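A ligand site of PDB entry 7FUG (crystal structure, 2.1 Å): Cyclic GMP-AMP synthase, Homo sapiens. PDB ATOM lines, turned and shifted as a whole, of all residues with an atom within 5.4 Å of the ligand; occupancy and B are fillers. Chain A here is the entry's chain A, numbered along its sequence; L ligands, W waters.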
ATOM      1  N   ARG A  86      33.403 -19.340  -5.890  1.00  0.00           N
ATOM      2  CA  ARG A  86      33.643 -18.161  -5.064  1.00  0.00           C
ATOM      3  C   ARG A  86      32.412 -17.291  -4.921  1.00  0.00           C
ATOM      4  O   ARG A  86      32.330 -16.466  -4.001  1.00  0.00           O
ATOM      5  CB  ARG A  86      34.786 -17.302  -5.621  1.00  0.00           C
ATOM      6  CG  ARG A  86      36.148 -17.986  -5.696  1.00  0.00           C
ATOM      7  CD  ARG A  86      36.985 -17.709  -4.447  1.00  0.00           C
ATOM      8  NE  ARG A  86      36.830 -18.767  -3.461  1.00  0.00           N
ATOM      9  CZ  ARG A  86      37.624 -19.827  -3.381  1.00  0.00           C
ATOM     10  NH1 ARG A  86      38.659 -19.965  -4.215  1.00  0.00           N
ATOM     11  NH2 ARG A  86      37.395 -20.755  -2.462  1.00  0.00           N
ATOM     12  N   ALA A  87      31.406 -17.527  -5.751  1.00  0.00           N
ATOM     13  CA  ALA A  87      30.255 -16.647  -5.807  1.00  0.00           C
ATOM     14  C   ALA A  87      28.938 -17.324  -5.428  1.00  0.00           C
ATOM     15  O   ALA A  87      28.022 -16.626  -4.977  1.00  0.00           O
ATOM     16  CB  ALA A  87      30.095 -16.061  -7.219  1.00  0.00           C
ATOM     17  N   TYR A  88      28.838 -18.632  -5.601  1.00  0.00           N
ATOM     18  CA  TYR A  88      27.611 -19.382  -5.361  1.00  0.00           C
ATOM     19  C   TYR A  88      27.754 -20.244  -4.132  1.00  0.00           C
ATOM     20  O   TYR A  88      28.839 -20.752  -3.830  1.00  0.00           O
ATOM     21  CB  TYR A  88      27.241 -20.221  -6.574  1.00  0.00           C
ATOM     22  CG  TYR A  88      27.168 -19.340  -7.785  1.00  0.00           C
ATOM     23  CD1 TYR A  88      26.046 -18.571  -8.027  1.00  0.00           C
ATOM     24  CD2 TYR A  88      28.253 -19.232  -8.653  1.00  0.00           C
ATOM     25  CE1 TYR A  88      25.975 -17.736  -9.126  1.00  0.00           C
ATOM     26  CE2 TYR A  88      28.187 -18.404  -9.756  1.00  0.00           C
ATOM     27  CZ  TYR A  88      27.048 -17.649  -9.993  1.00  0.00           C
ATOM     28  OH  TYR A  88      26.982 -16.808 -11.099  1.00  0.00           O
ATOM     29  N   LYS A 202      20.189 -17.679  -7.942  1.00  0.00           N
ATOM     30  CA  LYS A 202      20.735 -17.523  -9.278  1.00  0.00           C
ATOM     31  C   LYS A 202      21.406 -18.820  -9.693  1.00  0.00           C
ATOM     32  O   LYS A 202      22.307 -19.298  -8.998  1.00  0.00           O
ATOM     33  CB  LYS A 202      21.720 -16.345  -9.308  1.00  0.00           C
ATOM     34  CG  LYS A 202      21.977 -15.758 -10.709  1.00  0.00           C
ATOM     35  CD  LYS A 202      23.150 -16.457 -11.396  1.00  0.00           C
ATOM     36  CE  LYS A 202      23.264 -16.087 -12.875  1.00  0.00           C
ATOM     37  NZ  LYS A 202      24.059 -17.077 -13.683  1.00  0.00           N
ATOM     38  N   ARG A 216      23.558 -16.788  -4.493  1.00  0.00           N
ATOM     39  CA  ARG A 216      24.627 -15.925  -4.939  1.00  0.00           C
ATOM     40  C   ARG A 216      24.721 -14.695  -4.054  1.00  0.00           C
ATOM     41  O   ARG A 216      23.699 -14.149  -3.644  1.00  0.00           O
ATOM     42  CB  ARG A 216      24.375 -15.507  -6.361  1.00  0.00           C
ATOM     43  CG  ARG A 216      25.567 -14.917  -7.066  1.00  0.00           C
ATOM     44  CD  ARG A 216      25.039 -14.005  -8.146  1.00  0.00           C
ATOM     45  NE  ARG A 216      24.524 -12.784  -7.557  1.00  0.00           N
ATOM     46  CZ  ARG A 216      23.613 -12.002  -8.117  1.00  0.00           C
ATOM     47  NH1 ARG A 216      23.095 -12.327  -9.290  1.00  0.00           N
ATOM     48  NH2 ARG A 216      23.234 -10.903  -7.500  1.00  0.00           N
ATOM     49  N   LEU A 217      25.940 -14.266  -3.786  1.00  0.00           N
ATOM     50  CA  LEU A 217      26.143 -13.103  -2.925  1.00  0.00           C
ATOM     51  C   LEU A 217      25.636 -11.831  -3.579  1.00  0.00           C
ATOM     52  O   LEU A 217      25.714 -11.660  -4.797  1.00  0.00           O
ATOM     53  CB  LEU A 217      27.611 -12.958  -2.573  1.00  0.00           C
ATOM     54  CG  LEU A 217      28.157 -14.124  -1.762  1.00  0.00           C
ATOM     55  CD1 LEU A 217      29.597 -13.863  -1.395  1.00  0.00           C
ATOM     56  CD2 LEU A 217      27.310 -14.344  -0.520  1.00  0.00           C
ATOM     57  N   SER A 218      25.143 -10.918  -2.743  1.00  0.00           N
ATOM     58  CA  SER A 218      24.503  -9.701  -3.213  1.00  0.00           C
ATOM     59  C   SER A 218      24.815  -8.549  -2.258  1.00  0.00           C
ATOM     60  O   SER A 218      24.620  -8.672  -1.045  1.00  0.00           O
ATOM     61  CB  SER A 218      22.994  -9.922  -3.296  1.00  0.00           C
ATOM     62  OG  SER A 218      22.322  -8.757  -3.730  1.00  0.00           O
ATOM     63  N   PHE A 219      25.290  -7.446  -2.849  1.00  0.00           N
ATOM     64  CA  PHE A 219      25.746  -6.222  -2.193  1.00  0.00           C
ATOM     65  C   PHE A 219      25.084  -4.996  -2.817  1.00  0.00           C
ATOM     66  O   PHE A 219      25.685  -3.925  -2.891  1.00  0.00           O
ATOM     67  CB  PHE A 219      27.255  -6.073  -2.281  1.00  0.00           C
ATOM     68  CG  PHE A 219      28.010  -7.201  -1.634  1.00  0.00           C
ATOM     69  CD1 PHE A 219      28.212  -7.209  -0.284  1.00  0.00           C
ATOM     70  CD2 PHE A 219      28.474  -8.258  -2.393  1.00  0.00           C
ATOM     71  CE1 PHE A 219      28.883  -8.236   0.321  1.00  0.00           C
ATOM     72  CE2 PHE A 219      29.144  -9.281  -1.801  1.00  0.00           C
ATOM     73  CZ  PHE A 219      29.352  -9.279  -0.432  1.00  0.00           C
ATOM     74  N   SER A 220      23.829  -5.135  -3.278  1.00  0.00           N
ATOM     75  CA  SER A 220      23.117  -4.008  -3.882  1.00  0.00           C
ATOM     76  C   SER A 220      22.916  -2.845  -2.913  1.00  0.00           C
ATOM     77  O   SER A 220      22.788  -1.702  -3.344  1.00  0.00           O
ATOM     78  CB  SER A 220      21.762  -4.492  -4.381  1.00  0.00           C
ATOM     79  OG  SER A 220      21.139  -5.274  -3.376  1.00  0.00           O
ATOM     80  N   ILE A 222      25.251  -1.636  -1.077  1.00  0.00           N
ATOM     81  CA  ILE A 222      26.502  -0.911  -0.838  1.00  0.00           C
ATOM     82  C   ILE A 222      26.675   0.259  -1.807  1.00  0.00           C
ATOM     83  O   ILE A 222      27.258   1.277  -1.439  1.00  0.00           O
ATOM     84  CB  ILE A 222      27.714  -1.857  -0.924  1.00  0.00           C
ATOM     85  CG1 ILE A 222      27.639  -2.930   0.143  1.00  0.00           C
ATOM     86  CG2 ILE A 222      29.032  -1.094  -0.720  1.00  0.00           C
ATOM     87  CD1 ILE A 222      27.739  -2.388   1.566  1.00  0.00           C
ATOM     88  N   GLU A 223      26.170   0.111  -3.037  1.00  0.00           N
ATOM     89  CA  GLU A 223      26.278   1.176  -4.026  1.00  0.00           C
ATOM     90  C   GLU A 223      25.613   2.453  -3.520  1.00  0.00           C
ATOM     91  O   GLU A 223      26.143   3.556  -3.699  1.00  0.00           O
ATOM     92  CB  GLU A 223      25.652   0.731  -5.349  1.00  0.00           C
ATOM     93  CG  GLU A 223      25.624   1.760  -6.494  1.00  0.00           C
ATOM     94  CD  GLU A 223      24.707   1.333  -7.649  1.00  0.00           C
ATOM     95  OE1 GLU A 223      24.685   2.013  -8.695  1.00  0.00           O
ATOM     96  OE2 GLU A 223      23.997   0.312  -7.481  1.00  0.00           O
ATOM     97  N   ILE A 226      27.837   4.054  -0.779  1.00  0.00           N
ATOM     98  CA  ILE A 226      29.008   4.722  -1.363  1.00  0.00           C
ATOM     99  C   ILE A 226      28.594   6.004  -2.095  1.00  0.00           C
ATOM    100  O   ILE A 226      29.151   7.080  -1.848  1.00  0.00           O
ATOM    101  CB  ILE A 226      29.718   3.775  -2.331  1.00  0.00           C
ATOM    102  CG1 ILE A 226      30.479   2.687  -1.580  1.00  0.00           C
ATOM    103  CG2 ILE A 226      30.645   4.577  -3.197  1.00  0.00           C
ATOM    104  CD1 ILE A 226      31.253   1.762  -2.551  1.00  0.00           C
ATOM    105  N   TYR A 276      25.593  -3.722 -14.217  1.00  0.00           N
ATOM    106  CA  TYR A 276      26.529  -3.977 -13.148  1.00  0.00           C
ATOM    107  C   TYR A 276      27.942  -4.187 -13.678  1.00  0.00           C
ATOM    108  O   TYR A 276      28.897  -3.967 -12.933  1.00  0.00           O
ATOM    109  CB  TYR A 276      26.038  -5.137 -12.260  1.00  0.00           C
ATOM    110  CG  TYR A 276      26.310  -6.519 -12.763  1.00  0.00           C
ATOM    111  CD1 TYR A 276      25.440  -7.142 -13.647  1.00  0.00           C
ATOM    112  CD2 TYR A 276      27.437  -7.228 -12.342  1.00  0.00           C
ATOM    113  CE1 TYR A 276      25.708  -8.462 -14.119  1.00  0.00           C
ATOM    114  CE2 TYR A 276      27.712  -8.551 -12.794  1.00  0.00           C
ATOM    115  CZ  TYR A 276      26.841  -9.155 -13.692  1.00  0.00           C
ATOM    116  OH  TYR A 276      27.088 -10.449 -14.139  1.00  0.00           O
ATOM    117  N   LYS A 279      28.886  -0.497 -13.535  1.00  0.00           N
ATOM    118  CA  LYS A 279      29.156  -0.070 -12.164  1.00  0.00           C
ATOM    119  C   LYS A 279      30.490  -0.615 -11.681  1.00  0.00           C
ATOM    120  O   LYS A 279      31.296   0.103 -11.075  1.00  0.00           O
ATOM    121  CB  LYS A 279      28.035  -0.500 -11.247  1.00  0.00           C
ATOM    122  CG  LYS A 279      26.707   0.184 -11.461  1.00  0.00           C
ATOM    123  CD  LYS A 279      25.676  -0.620 -10.679  1.00  0.00           C
ATOM    124  CE  LYS A 279      24.242  -0.203 -10.940  1.00  0.00           C
ATOM    125  NZ  LYS A 279      23.291  -1.176 -10.271  1.00  0.00           N
ATOM    126  N   THR A 280      30.749  -1.903 -11.930  1.00  0.00           N
ATOM    127  CA  THR A 280      32.006  -2.458 -11.460  1.00  0.00           C
ATOM    128  C   THR A 280      33.171  -1.690 -12.044  1.00  0.00           C
ATOM    129  O   THR A 280      34.072  -1.266 -11.319  1.00  0.00           O
ATOM    130  CB  THR A 280      32.107  -3.928 -11.834  1.00  0.00           C
ATOM    131  OG1 THR A 280      31.015  -4.623 -11.205  1.00  0.00           O
ATOM    132  CG2 THR A 280      33.421  -4.494 -11.304  1.00  0.00           C
ATOM    133  N   PHE A 283      33.507   1.930 -10.348  1.00  0.00           N
ATOM    134  CA  PHE A 283      34.077   2.003  -9.014  1.00  0.00           C
ATOM    135  C   PHE A 283      35.537   1.551  -9.003  1.00  0.00           C
ATOM    136  O   PHE A 283      36.329   2.034  -8.173  1.00  0.00           O
ATOM    137  CB  PHE A 283      33.202   1.202  -8.061  1.00  0.00           C
ATOM    138  CG  PHE A 283      31.885   1.864  -7.823  1.00  0.00           C
ATOM    139  CD1 PHE A 283      31.825   3.045  -7.090  1.00  0.00           C
ATOM    140  CD2 PHE A 283      30.731   1.370  -8.354  1.00  0.00           C
ATOM    141  CE1 PHE A 283      30.623   3.678  -6.863  1.00  0.00           C
ATOM    142  CE2 PHE A 283      29.516   2.028  -8.147  1.00  0.00           C
ATOM    143  CZ  PHE A 283      29.479   3.183  -7.402  1.00  0.00           C
ATOM    144  N   ASN A 322      35.229  -8.590 -10.021  1.00  0.00           N
ATOM    145  CA  ASN A 322      34.081  -8.167  -9.225  1.00  0.00           C
ATOM    146  C   ASN A 322      34.548  -7.352  -8.035  1.00  0.00           C
ATOM    147  O   ASN A 322      35.587  -7.637  -7.436  1.00  0.00           O
ATOM    148  CB  ASN A 322      33.284  -9.401  -8.791  1.00  0.00           C
ATOM    149  CG  ASN A 322      32.162  -9.068  -7.857  1.00  0.00           C
ATOM    150  OD1 ASN A 322      32.393  -8.858  -6.662  1.00  0.00           O
ATOM    151  ND2 ASN A 322      30.943  -9.038  -8.379  1.00  0.00           N
ATOM    152  N   TYR A 323      33.798  -6.319  -7.689  1.00  0.00           N
ATOM    153  CA  TYR A 323      34.337  -5.342  -6.730  1.00  0.00           C
ATOM    154  C   TYR A 323      34.437  -5.958  -5.355  1.00  0.00           C
ATOM    155  O   TYR A 323      35.252  -5.537  -4.521  1.00  0.00           O
ATOM    156  CB  TYR A 323      33.444  -4.095  -6.712  1.00  0.00           C
ATOM    157  CG  TYR A 323      34.164  -2.825  -6.268  1.00  0.00           C
ATOM    158  CD1 TYR A 323      35.239  -2.326  -6.991  1.00  0.00           C
ATOM    159  CD2 TYR A 323      33.765  -2.133  -5.142  1.00  0.00           C
ATOM    160  CE1 TYR A 323      35.905  -1.161  -6.575  1.00  0.00           C
ATOM    161  CE2 TYR A 323      34.418  -0.972  -4.742  1.00  0.00           C
ATOM    162  CZ  TYR A 323      35.483  -0.499  -5.451  1.00  0.00           C
ATOM    163  OH  TYR A 323      36.121   0.639  -5.020  1.00  0.00           O
ATOM    164  N   PHE A 324      33.639  -6.995  -5.112  1.00  0.00           N
ATOM    165  CA  PHE A 324      33.574  -7.556  -3.782  1.00  0.00           C
ATOM    166  C   PHE A 324      34.308  -8.874  -3.658  1.00  0.00           C
ATOM    167  O   PHE A 324      34.816  -9.184  -2.582  1.00  0.00           O
ATOM    168  CB  PHE A 324      32.107  -7.736  -3.385  1.00  0.00           C
ATOM    169  CG  PHE A 324      31.350  -6.451  -3.407  1.00  0.00           C
ATOM    170  CD1 PHE A 324      31.315  -5.648  -2.286  1.00  0.00           C
ATOM    171  CD2 PHE A 324      30.704  -6.041  -4.558  1.00  0.00           C
ATOM    172  CE1 PHE A 324      30.646  -4.441  -2.312  1.00  0.00           C
ATOM    173  CE2 PHE A 324      30.029  -4.841  -4.579  1.00  0.00           C
ATOM    174  CZ  PHE A 324      29.999  -4.045  -3.461  1.00  0.00           C
ATOM    175  N   ILE A 325      34.373  -9.628  -4.747  1.00  0.00           N
ATOM    176  CA  ILE A 325      35.050 -10.918  -4.790  1.00  0.00           C
ATOM    177  C   ILE A 325      36.109 -10.791  -5.875  1.00  0.00           C
ATOM    178  O   ILE A 325      35.840 -11.118  -7.043  1.00  0.00           O
ATOM    179  CB  ILE A 325      34.059 -12.060  -5.049  1.00  0.00           C
ATOM    180  CG1 ILE A 325      33.164 -12.227  -3.830  1.00  0.00           C
ATOM    181  CG2 ILE A 325      34.777 -13.364  -5.175  1.00  0.00           C
ATOM    182  CD1 ILE A 325      31.701 -12.105  -4.091  1.00  0.00           C
ATOM    183  N   PHE A 328      36.773 -13.366  -8.829  1.00  0.00           N
ATOM    184  CA  PHE A 328      35.739 -13.687  -9.816  1.00  0.00           C
ATOM    185  C   PHE A 328      35.822 -12.675 -10.944  1.00  0.00           C
ATOM    186  O   PHE A 328      35.578 -11.487 -10.740  1.00  0.00           O
ATOM    187  CB  PHE A 328      34.337 -13.644  -9.212  1.00  0.00           C
ATOM    188  CG  PHE A 328      33.259 -14.139 -10.171  1.00  0.00           C
ATOM    189  CD1 PHE A 328      32.815 -13.336 -11.221  1.00  0.00           C
ATOM    190  CD2 PHE A 328      32.710 -15.413 -10.024  1.00  0.00           C
ATOM    191  CE1 PHE A 328      31.852 -13.804 -12.109  1.00  0.00           C
ATOM    192  CE2 PHE A 328      31.731 -15.899 -10.895  1.00  0.00           C
ATOM    193  CZ  PHE A 328      31.304 -15.096 -11.946  1.00  0.00           C
ATOM    194  N   LEU A 330      34.375 -11.064 -14.100  1.00  0.00           N
ATOM    195  CA  LEU A 330      33.156 -10.872 -14.888  1.00  0.00           C
ATOM    196  C   LEU A 330      33.391 -10.913 -16.390  1.00  0.00           C
ATOM    197  O   LEU A 330      32.430 -11.135 -17.142  1.00  0.00           O
ATOM    198  CB  LEU A 330      32.469  -9.530 -14.546  1.00  0.00           C
ATOM    199  CG  LEU A 330      32.158  -9.333 -13.049  1.00  0.00           C
ATOM    200  CD1 LEU A 330      31.657  -7.967 -12.786  1.00  0.00           C
ATOM    201  CD2 LEU A 330      31.126 -10.349 -12.580  1.00  0.00           C
HETATM  202  C1  LIG L   1      27.605  -4.745  -7.951  1.00  0.00           C
HETATM  203  C2  LIG L   1      27.637 -11.030  -8.402  1.00  0.00           C
HETATM  204  C3  LIG L   1      27.469 -11.501  -9.705  1.00  0.00           C
HETATM  205  C4  LIG L   1      28.458 -12.276 -10.280  1.00  0.00           C
HETATM  206  C5  LIG L   1      29.586 -12.611  -9.562  1.00  0.00           C
HETATM  207  C6  LIG L   1      29.742 -12.143  -8.275  1.00  0.00           C
HETATM  208  C7  LIG L   1      26.267 -11.128 -10.487  1.00  0.00           C
HETATM  209  C8  LIG L   1      25.717 -11.768 -11.616  1.00  0.00           C
HETATM  210  C9  LIG L   1      24.657 -11.006 -11.984  1.00  0.00           C
HETATM  211  C10 LIG L   1      23.666  -8.852 -11.113  1.00  0.00           C
HETATM  212  C11 LIG L   1      28.885  -2.708  -7.766  1.00  0.00           C
HETATM  213  C12 LIG L   1      30.277  -2.631  -7.797  1.00  0.00           C
HETATM  214  C13 LIG L   1      28.784 -11.337  -7.653  1.00  0.00           C
HETATM  215  C14 LIG L   1      27.962  -6.948  -7.147  1.00  0.00           C
HETATM  216  C15 LIG L   1      28.125  -3.577  -8.747  1.00  0.00           C
HETATM  217  C16 LIG L   1      28.971 -10.833  -6.241  1.00  0.00           C
HETATM  218  C17 LIG L   1      30.963  -1.849  -6.896  1.00  0.00           C
HETATM  219  C18 LIG L   1      30.287  -1.119  -5.943  1.00  0.00           C
HETATM  220  C19 LIG L   1      28.901  -1.167  -5.909  1.00  0.00           C
HETATM  221  C20 LIG L   1      28.215  -1.963  -6.807  1.00  0.00           C
HETATM  222  C21 LIG L   1      27.634  -8.757  -6.169  1.00  0.00           C
HETATM  223  C22 LIG L   1      25.884  -5.806  -6.571  1.00  0.00           C
HETATM  224  C23 LIG L   1      26.389  -4.713  -7.340  1.00  0.00           C
HETATM  225  N1  LIG L   1      28.383  -5.874  -7.858  1.00  0.00           N
HETATM  226  N2  LIG L   1      28.555  -8.121  -6.960  1.00  0.00           N
HETATM  227  N3  LIG L   1      24.616  -9.954 -11.126  1.00  0.00           N
HETATM  228  N4  LIG L   1      25.600  -9.997 -10.201  1.00  0.00           N
HETATM  229  N5  LIG L   1      27.868 -10.040  -5.720  1.00  0.00           N
HETATM  230  N6  LIG L   1      26.523  -8.097  -5.877  1.00  0.00           N
HETATM  231  N7  LIG L   1      26.763  -6.893  -6.529  1.00  0.00           N
HETATM  232  O1  LIG L   1      24.794  -5.860  -5.970  1.00  0.00           O
HETATM  233 CL1  LIG L   1      31.185 -12.579  -7.418  1.00  0.00          CL
HETATM  234  O   HOH W   1      31.503  -5.837  -8.837  1.00  0.00           O
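N5 of the ligand is in hydrogen-bond range of O of Leu 217 (2.8 Å). A nitrogen (N2) of the ligand sits at hydrogen-bond distance from the side-chain amide nitrogen (ND2) of Asn 322. The backbone NH (N) of Ser 220 sits at hydrogen-bond distance from an oxygen (O1) of the ligand, 3.0 Å away. N6 of the ligand is in hydrogen-bond range of N of Phe 219 (3.3 Å).
The guanidinium group (NH1) of Arg 216 sits close to a nitrogen (N3) of the ligand, at 3.4 Å. CB of Ala 87 touches CL1 of the ligand, 3.7 Å away. Ser 218 touches the ligand. CB of Glu 223 touches C19 of the ligand, 3.8 Å away. Tyr 276 touches the ligand (OH to C8, 3.2 Å). CB of Lys 279 touches C15 of the ligand, at 3.97 Å. OG1 of Thr 280 touches C15 of the ligand, 3.9 Å away. CD2 of Phe 283 touches C18 of the ligand, 3.5 Å away. Tyr 323 touches the ligand. Phe 324 touches the ligand. Ile 325 touches the ligand. CE1 of Phe 328 touches C5 of the ligand (3.6 Å). Hydrophobic or aromatic side chains within 4 Å of the ligand: Ala 87, Phe 219, Tyr 276, Phe 283, Tyr 323, Phe 324, Ile 325 and Phe 328. 16 residues have an atom within 4 Å of the ligand: Ala 87, Arg 216, Leu 217, Ser 218, Phe 219, Ser 220, Glu 223, Tyr 276, Lys 279, Thr 280, Phe 283, Asn 322, Tyr 323, Phe 324, Ile 325 and Phe 328. Along chain A the residues within 4 Å of the ligand span positions 87 to 328.
The backbone NH (N) of Leu 217 is in hydrogen-bond range of the backbone carbonyl oxygen (O) of Ala 87 (3.4 Å). The side-chain amide oxygen (OD1) of Asn 322 lies within hydrogen-bond range of the backbone NH (N) of Ile 325 (2.9 Å). N of Asn 322 lies within hydrogen-bond range of O of Phe 328. The side-chain amide oxygen (OD1) of Asn 322 is in hydrogen-bond range of the backbone NH (N) of Phe 324 (2.7 Å). The side-chain hydroxyl of Thr 280 lies within hydrogen-bond range of the backbone carbonyl oxygen of Tyr 276 (2.8 Å). OH of Tyr 323 sits at hydrogen-bond distance from O of Phe 283, 3.5 Å away. OE2 of Glu 223 lies within salt-bridge range of NZ of Lys 279, 3.2 Å away.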
